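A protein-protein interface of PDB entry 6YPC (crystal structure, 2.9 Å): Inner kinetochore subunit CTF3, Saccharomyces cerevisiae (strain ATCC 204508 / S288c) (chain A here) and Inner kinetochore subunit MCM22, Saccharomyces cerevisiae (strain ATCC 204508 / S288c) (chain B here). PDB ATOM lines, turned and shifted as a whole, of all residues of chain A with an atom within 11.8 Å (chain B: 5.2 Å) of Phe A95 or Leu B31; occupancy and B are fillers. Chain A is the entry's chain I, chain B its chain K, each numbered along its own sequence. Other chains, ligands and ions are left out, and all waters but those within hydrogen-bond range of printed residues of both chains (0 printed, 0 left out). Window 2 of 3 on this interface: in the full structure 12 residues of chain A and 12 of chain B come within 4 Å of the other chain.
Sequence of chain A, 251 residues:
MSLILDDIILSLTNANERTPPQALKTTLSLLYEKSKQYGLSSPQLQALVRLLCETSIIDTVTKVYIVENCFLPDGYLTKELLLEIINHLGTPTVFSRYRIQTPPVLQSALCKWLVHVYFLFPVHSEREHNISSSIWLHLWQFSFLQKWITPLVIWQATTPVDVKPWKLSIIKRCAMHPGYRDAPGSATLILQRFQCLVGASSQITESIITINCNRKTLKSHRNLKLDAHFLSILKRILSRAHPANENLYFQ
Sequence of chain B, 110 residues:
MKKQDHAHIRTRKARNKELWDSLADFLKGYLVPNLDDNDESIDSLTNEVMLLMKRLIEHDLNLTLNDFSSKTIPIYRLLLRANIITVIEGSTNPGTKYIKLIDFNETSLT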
ATOM      1  N   ASN A  87      -5.108  -3.038  -0.677  1.00  0.00           N
ATOM      2  CA  ASN A  87      -5.732  -2.846  -1.964  1.00  0.00           C
ATOM      3  C   ASN A  87      -4.794  -2.151  -2.945  1.00  0.00           C
ATOM      4  O   ASN A  87      -5.121  -2.023  -4.125  1.00  0.00           O
ATOM      5  CB  ASN A  87      -7.027  -2.080  -1.776  1.00  0.00           C
ATOM      6  CG  ASN A  87      -8.169  -2.995  -1.454  1.00  0.00           C
ATOM      7  OD1 ASN A  87      -8.258  -4.067  -2.017  1.00  0.00           O
ATOM      8  ND2 ASN A  87      -9.054  -2.580  -0.564  1.00  0.00           N
ATOM      9  N   GLY A  90       0.465  -5.518  -5.153  1.00  0.00           N
ATOM     10  CA  GLY A  90       0.380  -6.526  -6.180  1.00  0.00           C
ATOM     11  C   GLY A  90       0.963  -6.039  -7.492  1.00  0.00           C
ATOM     12  O   GLY A  90       1.763  -5.098  -7.535  1.00  0.00           O
ATOM     13  N   THR A  91       0.554  -6.710  -8.569  1.00  0.00           N
ATOM     14  CA  THR A  91       0.998  -6.543  -9.938  1.00  0.00           C
ATOM     15  C   THR A  91      -0.212  -6.283 -10.836  1.00  0.00           C
ATOM     16  O   THR A  91      -1.328  -6.733 -10.533  1.00  0.00           O
ATOM     17  CB  THR A  91       1.743  -7.800 -10.413  1.00  0.00           C
ATOM     18  OG1 THR A  91       2.286  -7.590 -11.718  1.00  0.00           O
ATOM     19  CG2 THR A  91       0.788  -8.985 -10.484  1.00  0.00           C
ATOM     20  N   PRO A  92      -0.038  -5.539 -11.930  1.00  0.00           N
ATOM     21  CA  PRO A  92      -1.143  -5.360 -12.881  1.00  0.00           C
ATOM     22  C   PRO A  92      -1.424  -6.654 -13.629  1.00  0.00           C
ATOM     23  O   PRO A  92      -0.523  -7.250 -14.219  1.00  0.00           O
ATOM     24  CB  PRO A  92      -0.625  -4.275 -13.828  1.00  0.00           C
ATOM     25  CG  PRO A  92       0.571  -3.715 -13.158  1.00  0.00           C
ATOM     26  CD  PRO A  92       1.156  -4.797 -12.347  1.00  0.00           C
ATOM     27  N   THR A  93      -2.679  -7.078 -13.621  1.00  0.00           N
ATOM     28  CA  THR A  93      -3.033  -8.346 -14.229  1.00  0.00           C
ATOM     29  C   THR A  93      -4.065  -8.146 -15.336  1.00  0.00           C
ATOM     30  O   THR A  93      -4.682  -7.087 -15.453  1.00  0.00           O
ATOM     31  CB  THR A  93      -3.553  -9.323 -13.168  1.00  0.00           C
ATOM     32  OG1 THR A  93      -3.785 -10.593 -13.790  1.00  0.00           O
ATOM     33  CG2 THR A  93      -4.845  -8.839 -12.585  1.00  0.00           C
ATOM     34  N   VAL A  94      -4.261  -9.190 -16.142  1.00  0.00           N
ATOM     35  CA  VAL A  94      -5.130  -9.125 -17.315  1.00  0.00           C
ATOM     36  C   VAL A  94      -6.556  -8.713 -16.956  1.00  0.00           C
ATOM     37  O   VAL A  94      -7.337  -8.332 -17.835  1.00  0.00           O
ATOM     38  CB  VAL A  94      -5.144 -10.460 -18.086  1.00  0.00           C
ATOM     39  CG1 VAL A  94      -3.775 -10.748 -18.676  1.00  0.00           C
ATOM     40  CG2 VAL A  94      -5.587 -11.593 -17.196  1.00  0.00           C
ATOM     41  N   PHE A  95      -6.927  -8.791 -15.690  1.00  0.00           N
ATOM     42  CA  PHE A  95      -8.226  -8.261 -15.299  1.00  0.00           C
ATOM     43  C   PHE A  95      -8.120  -6.852 -14.743  1.00  0.00           C
ATOM     44  O   PHE A  95      -9.135  -6.279 -14.333  1.00  0.00           O
ATOM     45  CB  PHE A  95      -8.915  -9.159 -14.256  1.00  0.00           C
ATOM     46  CG  PHE A  95      -9.021 -10.612 -14.646  1.00  0.00           C
ATOM     47  CD1 PHE A  95      -7.909 -11.439 -14.634  1.00  0.00           C
ATOM     48  CD2 PHE A  95     -10.233 -11.154 -14.969  1.00  0.00           C
ATOM     49  CE1 PHE A  95      -7.995 -12.764 -14.972  1.00  0.00           C
ATOM     50  CE2 PHE A  95     -10.325 -12.486 -15.319  1.00  0.00           C
ATOM     51  CZ  PHE A  95      -9.197 -13.289 -15.323  1.00  0.00           C
ATOM     52  N   SER A  96      -6.916  -6.289 -14.721  1.00  0.00           N
ATOM     53  CA  SER A  96      -6.633  -5.099 -13.936  1.00  0.00           C
ATOM     54  C   SER A  96      -5.589  -4.255 -14.655  1.00  0.00           C
ATOM     55  O   SER A  96      -4.660  -3.715 -14.052  1.00  0.00           O
ATOM     56  CB  SER A  96      -6.200  -5.497 -12.523  1.00  0.00           C
ATOM     57  OG  SER A  96      -4.803  -5.751 -12.401  1.00  0.00           O
ATOM     58  N   ARG A  97      -5.759  -4.104 -15.969  1.00  0.00           N
ATOM     59  CA  ARG A  97      -4.784  -3.348 -16.748  1.00  0.00           C
ATOM     60  C   ARG A  97      -5.067  -1.848 -16.717  1.00  0.00           C
ATOM     61  O   ARG A  97      -4.132  -1.048 -16.819  1.00  0.00           O
ATOM     62  CB  ARG A  97      -4.720  -3.877 -18.187  1.00  0.00           C
ATOM     63  CG  ARG A  97      -5.868  -3.464 -19.098  1.00  0.00           C
ATOM     64  CD  ARG A  97      -5.543  -2.181 -19.900  1.00  0.00           C
ATOM     65  NE  ARG A  97      -6.585  -1.845 -20.874  1.00  0.00           N
ATOM     66  CZ  ARG A  97      -7.522  -0.910 -20.704  1.00  0.00           C
ATOM     67  NH1 ARG A  97      -7.572  -0.196 -19.582  1.00  0.00           N
ATOM     68  NH2 ARG A  97      -8.419  -0.693 -21.661  1.00  0.00           N
ATOM     69  N   TYR A  98      -6.334  -1.459 -16.570  1.00  0.00           N
ATOM     70  CA  TYR A  98      -6.799  -0.096 -16.329  1.00  0.00           C
ATOM     71  C   TYR A  98      -6.447   0.431 -14.935  1.00  0.00           C
ATOM     72  O   TYR A  98      -6.843   1.556 -14.589  1.00  0.00           O
ATOM     73  CB  TYR A  98      -8.317  -0.063 -16.484  1.00  0.00           C
ATOM     74  CG  TYR A  98      -9.016  -0.947 -15.436  1.00  0.00           C
ATOM     75  CD1 TYR A  98      -8.945  -2.359 -15.520  1.00  0.00           C
ATOM     76  CD2 TYR A  98      -9.729  -0.381 -14.352  1.00  0.00           C
ATOM     77  CE1 TYR A  98      -9.556  -3.178 -14.572  1.00  0.00           C
ATOM     78  CE2 TYR A  98     -10.355  -1.204 -13.395  1.00  0.00           C
ATOM     79  CZ  TYR A  98     -10.261  -2.603 -13.525  1.00  0.00           C
ATOM     80  OH  TYR A  98     -10.852  -3.449 -12.617  1.00  0.00           O
ATOM     81  N   ARG A  99      -5.766  -0.355 -14.110  1.00  0.00           N
ATOM     82  CA  ARG A  99      -5.601  -0.030 -12.709  1.00  0.00           C
ATOM     83  C   ARG A  99      -4.417   0.920 -12.545  1.00  0.00           C
ATOM     84  O   ARG A  99      -3.436   0.846 -13.295  1.00  0.00           O
ATOM     85  CB  ARG A  99      -5.417  -1.327 -11.908  1.00  0.00           C
ATOM     86  CG  ARG A  99      -5.239  -1.193 -10.395  1.00  0.00           C
ATOM     87  CD  ARG A  99      -4.968  -2.568  -9.767  1.00  0.00           C
ATOM     88  NE  ARG A  99      -4.828  -2.499  -8.310  1.00  0.00           N
ATOM     89  CZ  ARG A  99      -4.344  -3.479  -7.544  1.00  0.00           C
ATOM     90  NH1 ARG A  99      -4.252  -3.315  -6.226  1.00  0.00           N
ATOM     91  NH2 ARG A  99      -3.927  -4.616  -8.089  1.00  0.00           N
ATOM     92  N   ILE A 100      -4.543   1.857 -11.608  1.00  0.00           N
ATOM     93  CA  ILE A 100      -3.401   2.663 -11.196  1.00  0.00           C
ATOM     94  C   ILE A 100      -2.492   1.737 -10.400  1.00  0.00           C
ATOM     95  O   ILE A 100      -2.866   1.301  -9.309  1.00  0.00           O
ATOM     96  CB  ILE A 100      -3.828   3.868 -10.347  1.00  0.00           C
ATOM     97  CG1 ILE A 100      -5.178   4.427 -10.807  1.00  0.00           C
ATOM     98  CG2 ILE A 100      -2.729   4.927 -10.349  1.00  0.00           C
ATOM     99  CD1 ILE A 100      -5.794   5.427  -9.830  1.00  0.00           C
ATOM    100  N   GLN A 101      -1.318   1.405 -10.929  1.00  0.00           N
ATOM    101  CA  GLN A 101      -0.476   0.546 -10.110  1.00  0.00           C
ATOM    102  C   GLN A 101       0.706   1.307  -9.547  1.00  0.00           C
ATOM    103  O   GLN A 101       1.195   2.277 -10.130  1.00  0.00           O
ATOM    104  CB  GLN A 101      -0.002  -0.713 -10.835  1.00  0.00           C
ATOM    105  CG  GLN A 101      -0.760  -1.969 -10.280  1.00  0.00           C
ATOM    106  CD  GLN A 101      -0.402  -2.296  -8.804  1.00  0.00           C
ATOM    107  OE1 GLN A 101       0.744  -2.636  -8.499  1.00  0.00           O
ATOM    108  NE2 GLN A 101      -1.381  -2.159  -7.891  1.00  0.00           N
ATOM    109  N   PHE B  26     -19.487 -11.097  -6.962  1.00  0.00           N
ATOM    110  CA  PHE B  26     -18.155 -10.708  -7.392  1.00  0.00           C
ATOM    111  C   PHE B  26     -17.857 -11.166  -8.806  1.00  0.00           C
ATOM    112  O   PHE B  26     -17.041 -10.548  -9.495  1.00  0.00           O
ATOM    113  CB  PHE B  26     -17.133 -11.292  -6.442  1.00  0.00           C
ATOM    114  CG  PHE B  26     -15.779 -11.425  -7.026  1.00  0.00           C
ATOM    115  CD1 PHE B  26     -14.905 -10.371  -6.988  1.00  0.00           C
ATOM    116  CD2 PHE B  26     -15.367 -12.611  -7.585  1.00  0.00           C
ATOM    117  CE1 PHE B  26     -13.645 -10.481  -7.501  1.00  0.00           C
ATOM    118  CE2 PHE B  26     -14.105 -12.730  -8.098  1.00  0.00           C
ATOM    119  CZ  PHE B  26     -13.236 -11.662  -8.057  1.00  0.00           C
ATOM    120  N   LEU B  27     -18.437 -12.285  -9.228  1.00  0.00           N
ATOM    121  CA  LEU B  27     -18.208 -12.745 -10.590  1.00  0.00           C
ATOM    122  C   LEU B  27     -18.974 -11.882 -11.561  1.00  0.00           C
ATOM    123  O   LEU B  27     -18.407 -11.317 -12.503  1.00  0.00           O
ATOM    124  CB  LEU B  27     -18.639 -14.195 -10.749  1.00  0.00           C
ATOM    125  CG  LEU B  27     -17.783 -15.263 -10.116  1.00  0.00           C
ATOM    126  CD1 LEU B  27     -18.337 -16.594 -10.566  1.00  0.00           C
ATOM    127  CD2 LEU B  27     -16.349 -15.080 -10.578  1.00  0.00           C
ATOM    128  N   GLY B  29     -20.168  -9.052 -11.041  1.00  0.00           N
ATOM    129  CA  GLY B  29     -19.781  -7.670 -10.843  1.00  0.00           C
ATOM    130  C   GLY B  29     -18.409  -7.275 -11.355  1.00  0.00           C
ATOM    131  O   GLY B  29     -18.272  -6.219 -11.975  1.00  0.00           O
ATOM    132  N   TYR B  30     -17.386  -8.096 -11.113  1.00  0.00           N
ATOM    133  CA  TYR B  30     -16.014  -7.718 -11.437  1.00  0.00           C
ATOM    134  C   TYR B  30     -15.305  -8.696 -12.351  1.00  0.00           C
ATOM    135  O   TYR B  30     -14.703  -8.275 -13.342  1.00  0.00           O
ATOM    136  CB  TYR B  30     -15.191  -7.574 -10.172  1.00  0.00           C
ATOM    137  CG  TYR B  30     -13.727  -7.291 -10.420  1.00  0.00           C
ATOM    138  CD1 TYR B  30     -13.259  -5.992 -10.538  1.00  0.00           C
ATOM    139  CD2 TYR B  30     -12.809  -8.313 -10.493  1.00  0.00           C
ATOM    140  CE1 TYR B  30     -11.915  -5.739 -10.741  1.00  0.00           C
ATOM    141  CE2 TYR B  30     -11.464  -8.066 -10.695  1.00  0.00           C
ATOM    142  CZ  TYR B  30     -11.025  -6.782 -10.820  1.00  0.00           C
ATOM    143  OH  TYR B  30      -9.685  -6.553 -11.030  1.00  0.00           O
ATOM    144  N   LEU B  31     -15.321  -9.990 -12.035  1.00  0.00           N
ATOM    145  CA  LEU B  31     -14.395 -10.896 -12.704  1.00  0.00           C
ATOM    146  C   LEU B  31     -14.787 -11.159 -14.146  1.00  0.00           C
ATOM    147  O   LEU B  31     -13.921 -11.225 -15.024  1.00  0.00           O
ATOM    148  CB  LEU B  31     -14.306 -12.205 -11.949  1.00  0.00           C
ATOM    149  CG  LEU B  31     -13.127 -13.030 -12.434  1.00  0.00           C
ATOM    150  CD1 LEU B  31     -11.854 -12.258 -12.241  1.00  0.00           C
ATOM    151  CD2 LEU B  31     -13.067 -14.326 -11.648  1.00  0.00           C
ATOM    152  N   VAL B  32     -16.076 -11.348 -14.402  1.00  0.00           N
ATOM    153  CA  VAL B  32     -16.563 -11.733 -15.726  1.00  0.00           C
ATOM    154  C   VAL B  32     -16.611 -10.514 -16.642  1.00  0.00           C
ATOM    155  O   VAL B  32     -16.207 -10.620 -17.808  1.00  0.00           O
ATOM    156  CB  VAL B  32     -17.934 -12.426 -15.630  1.00  0.00           C
ATOM    157  CG1 VAL B  32     -18.320 -13.041 -16.953  1.00  0.00           C
ATOM    158  CG2 VAL B  32     -17.905 -13.496 -14.552  1.00  0.00           C
ATOM    159  N   PRO B  33     -17.074  -9.349 -16.173  1.00  0.00           N
ATOM    160  CA  PRO B  33     -16.943  -8.134 -16.999  1.00  0.00           C
ATOM    161  C   PRO B  33     -15.515  -7.828 -17.433  1.00  0.00           C
ATOM    162  O   PRO B  33     -15.309  -7.329 -18.544  1.00  0.00           O
ATOM    163  CB  PRO B  33     -17.485  -7.032 -16.088  1.00  0.00           C
ATOM    164  CG  PRO B  33     -18.373  -7.725 -15.120  1.00  0.00           C
ATOM    165  CD  PRO B  33     -17.795  -9.076 -14.912  1.00  0.00           C
ATOM    166  N   ASN B  34     -14.517  -8.095 -16.602  1.00  0.00           N
ATOM    167  CA  ASN B  34     -13.151  -7.866 -17.048  1.00  0.00           C
ATOM    168  C   ASN B  34     -12.633  -8.981 -17.933  1.00  0.00           C
ATOM    169  O   ASN B  34     -11.472  -8.921 -18.360  1.00  0.00           O
ATOM    170  CB  ASN B  34     -12.237  -7.669 -15.847  1.00  0.00           C
ATOM    171  CG  ASN B  34     -12.403  -6.286 -15.235  1.00  0.00           C
ATOM    172  OD1 ASN B  34     -12.292  -5.267 -15.924  1.00  0.00           O
ATOM    173  ND2 ASN B  34     -12.710  -6.244 -13.949  1.00  0.00           N
ATOM    174  N   LEU B  35     -13.455 -10.006 -18.189  1.00  0.00           N
ATOM    175  CA  LEU B  35     -13.180 -10.929 -19.284  1.00  0.00           C
ATOM    176  C   LEU B  35     -13.657 -10.334 -20.609  1.00  0.00           C
ATOM    177  O   LEU B  35     -12.926 -10.388 -21.605  1.00  0.00           O
ATOM    178  CB  LEU B  35     -13.850 -12.289 -19.025  1.00  0.00           C
ATOM    179  CG  LEU B  35     -13.195 -13.432 -18.225  1.00  0.00           C
ATOM    180  CD1 LEU B  35     -14.171 -14.551 -17.994  1.00  0.00           C
ATOM    181  CD2 LEU B  35     -12.008 -13.992 -18.936  1.00  0.00           C
ATOM    182  N   PRO B  74      -8.765 -17.611 -19.365  1.00  0.00           N
ATOM    183  CA  PRO B  74      -8.006 -16.802 -18.397  1.00  0.00           C
ATOM    184  C   PRO B  74      -8.265 -17.221 -16.979  1.00  0.00           C
ATOM    185  O   PRO B  74      -7.318 -17.304 -16.194  1.00  0.00           O
ATOM    186  CB  PRO B  74      -8.493 -15.372 -18.647  1.00  0.00           C
ATOM    187  CG  PRO B  74      -8.979 -15.384 -20.008  1.00  0.00           C
ATOM    188  CD  PRO B  74      -9.575 -16.734 -20.231  1.00  0.00           C
ATOM    189  N   ILE B  75      -9.529 -17.493 -16.640  1.00  0.00           N
ATOM    190  CA  ILE B  75      -9.860 -18.021 -15.316  1.00  0.00           C
ATOM    191  C   ILE B  75      -8.885 -19.122 -14.937  1.00  0.00           C
ATOM    192  O   ILE B  75      -8.183 -19.045 -13.919  1.00  0.00           O
ATOM    193  CB  ILE B  75     -11.303 -18.544 -15.283  1.00  0.00           C
ATOM    194  CG1 ILE B  75     -12.252 -17.410 -15.573  1.00  0.00           C
ATOM    195  CG2 ILE B  75     -11.600 -19.079 -13.915  1.00  0.00           C
ATOM    196  CD1 ILE B  75     -12.164 -16.332 -14.534  1.00  0.00           C
ATOM    197  N   LEU B  78      -5.714 -17.821 -14.203  1.00  0.00           N
ATOM    198  CA  LEU B  78      -5.703 -17.067 -12.960  1.00  0.00           C
ATOM    199  C   LEU B  78      -5.539 -18.004 -11.774  1.00  0.00           C
ATOM    200  O   LEU B  78      -4.731 -17.750 -10.868  1.00  0.00           O
ATOM    201  CB  LEU B  78      -6.992 -16.260 -12.849  1.00  0.00           C
ATOM    202  CG  LEU B  78      -7.404 -15.808 -11.460  1.00  0.00           C
ATOM    203  CD1 LEU B  78      -6.553 -14.633 -11.073  1.00  0.00           C
ATOM    204  CD2 LEU B  78      -8.883 -15.431 -11.440  1.00  0.00           C
ATOM    205  N   ARG B  81      -1.952 -19.125 -11.693  1.00  0.00           N
ATOM    206  CA  ARG B  81      -1.008 -18.154 -11.146  1.00  0.00           C
ATOM    207  C   ARG B  81      -1.054 -18.139  -9.629  1.00  0.00           C
ATOM    208  O   ARG B  81      -0.006 -18.171  -8.964  1.00  0.00           O
ATOM    209  CB  ARG B  81      -1.302 -16.756 -11.689  1.00  0.00           C
ATOM    210  CG  ARG B  81      -0.399 -16.350 -12.827  1.00  0.00           C
ATOM    211  CD  ARG B  81      -0.685 -14.956 -13.286  1.00  0.00           C
ATOM    212  NE  ARG B  81      -2.074 -14.841 -13.684  1.00  0.00           N
ATOM    213  CZ  ARG B  81      -2.951 -14.053 -13.078  1.00  0.00           C
ATOM    214  NH1 ARG B  81      -2.560 -13.301 -12.048  1.00  0.00           N
ATOM    215  NH2 ARG B  81      -4.214 -14.021 -13.503  1.00  0.00           N
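The backbone carbonyl oxygen of Phe A95 lies within hydrogen-bond range of the side-chain hydroxyl of Tyr B30 (3.4 Å). NH1 of Arg B81 is in hydrogen-bond range of OG1 of Thr A93.
N of Leu B31 is in hydrogen-bond range of O of Phe B26, 3.1 Å away. The backbone carbonyl oxygen (O) of Tyr B30 sits at hydrogen-bond distance from the side-chain amide nitrogen (ND2) of Asn B34 (2.9 Å). The backbone NH (N) of Thr A93 lies within hydrogen-bond range of the side-chain hydroxyl (OG) of Ser A96.
CD1 of Leu B31 touches CD2 of Phe A95, 3.4 Å away. Phe A95 touches Asn B34. CB of Pro B74 touches CZ of Phe A95, 3.99 Å away. CB of Ser A96 touches OH of Tyr B30, 3.9 Å away. Tyr A98 touches Tyr B30 (OH to CE1, 3.1 Å). ND2 of Asn B34 touches OH of Tyr A98, at 3.6 Å.
Printed residues of chain B within 4 Å of Thr A93: Arg B81. Printed residues of chain B within 4 Å of Phe A95: Tyr B30 (3.4 Å), Leu B31 (3.4 Å), Asn B34 (3.4 Å) and Pro B74 (3.99 Å). Of the printed residues of chain B, Tyr A98 touches Tyr B30 (3.1 Å) and Asn B34 (3.6 Å). Ile A100 touches none of the printed residues of chain B. No residue of chain A comes within 4 Å of Phe B26. No residue of chain A comes within 4 Å of Leu B27. No residue of chain A comes within 4 Å of Gly B29. Tyr B30 touches just these residues of chain A: Phe A95, Ser A96 and Tyr A98. Leu B31 touches just one residue of chain A: Phe A95 (3.4 Å). No residue of chain A comes within 4 Å of Val B32. No residue of chain A comes within 4 Å of Pro B33. Of chain A, only Phe A95 (3.4 Å) and Tyr A98 (3.6 Å) come within 4 Å of Asn B34. No residue of chain A comes within 4 Å of Leu B35. Of the printed residues of chain A, Pro B74 touches Phe A95 (3.99 Å). No residue of chain A comes within 4 Å of Ile B75. The nearest printed residue of chain B that does not touch Phe A95 is Leu B35 (4.2 Å).
Printed residues of chain A that touch a printed residue of chain B: Thr A93, Phe A95, Ser A96 and Tyr A98. Of the 13 printed residues of chain B, 5 touch a printed residue of chain A. Hydrophobic or aromatic side chains of chain B within 4 Å of the printed part of chain A: Tyr B30, Leu B31 and Pro B74. Among the printed residues, 8 pairs touch across the chains. Among the printed residues, no Asp or Glu carboxylate lies within 4 Å of a Lys or Arg side-chain nitrogen of the other chain.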
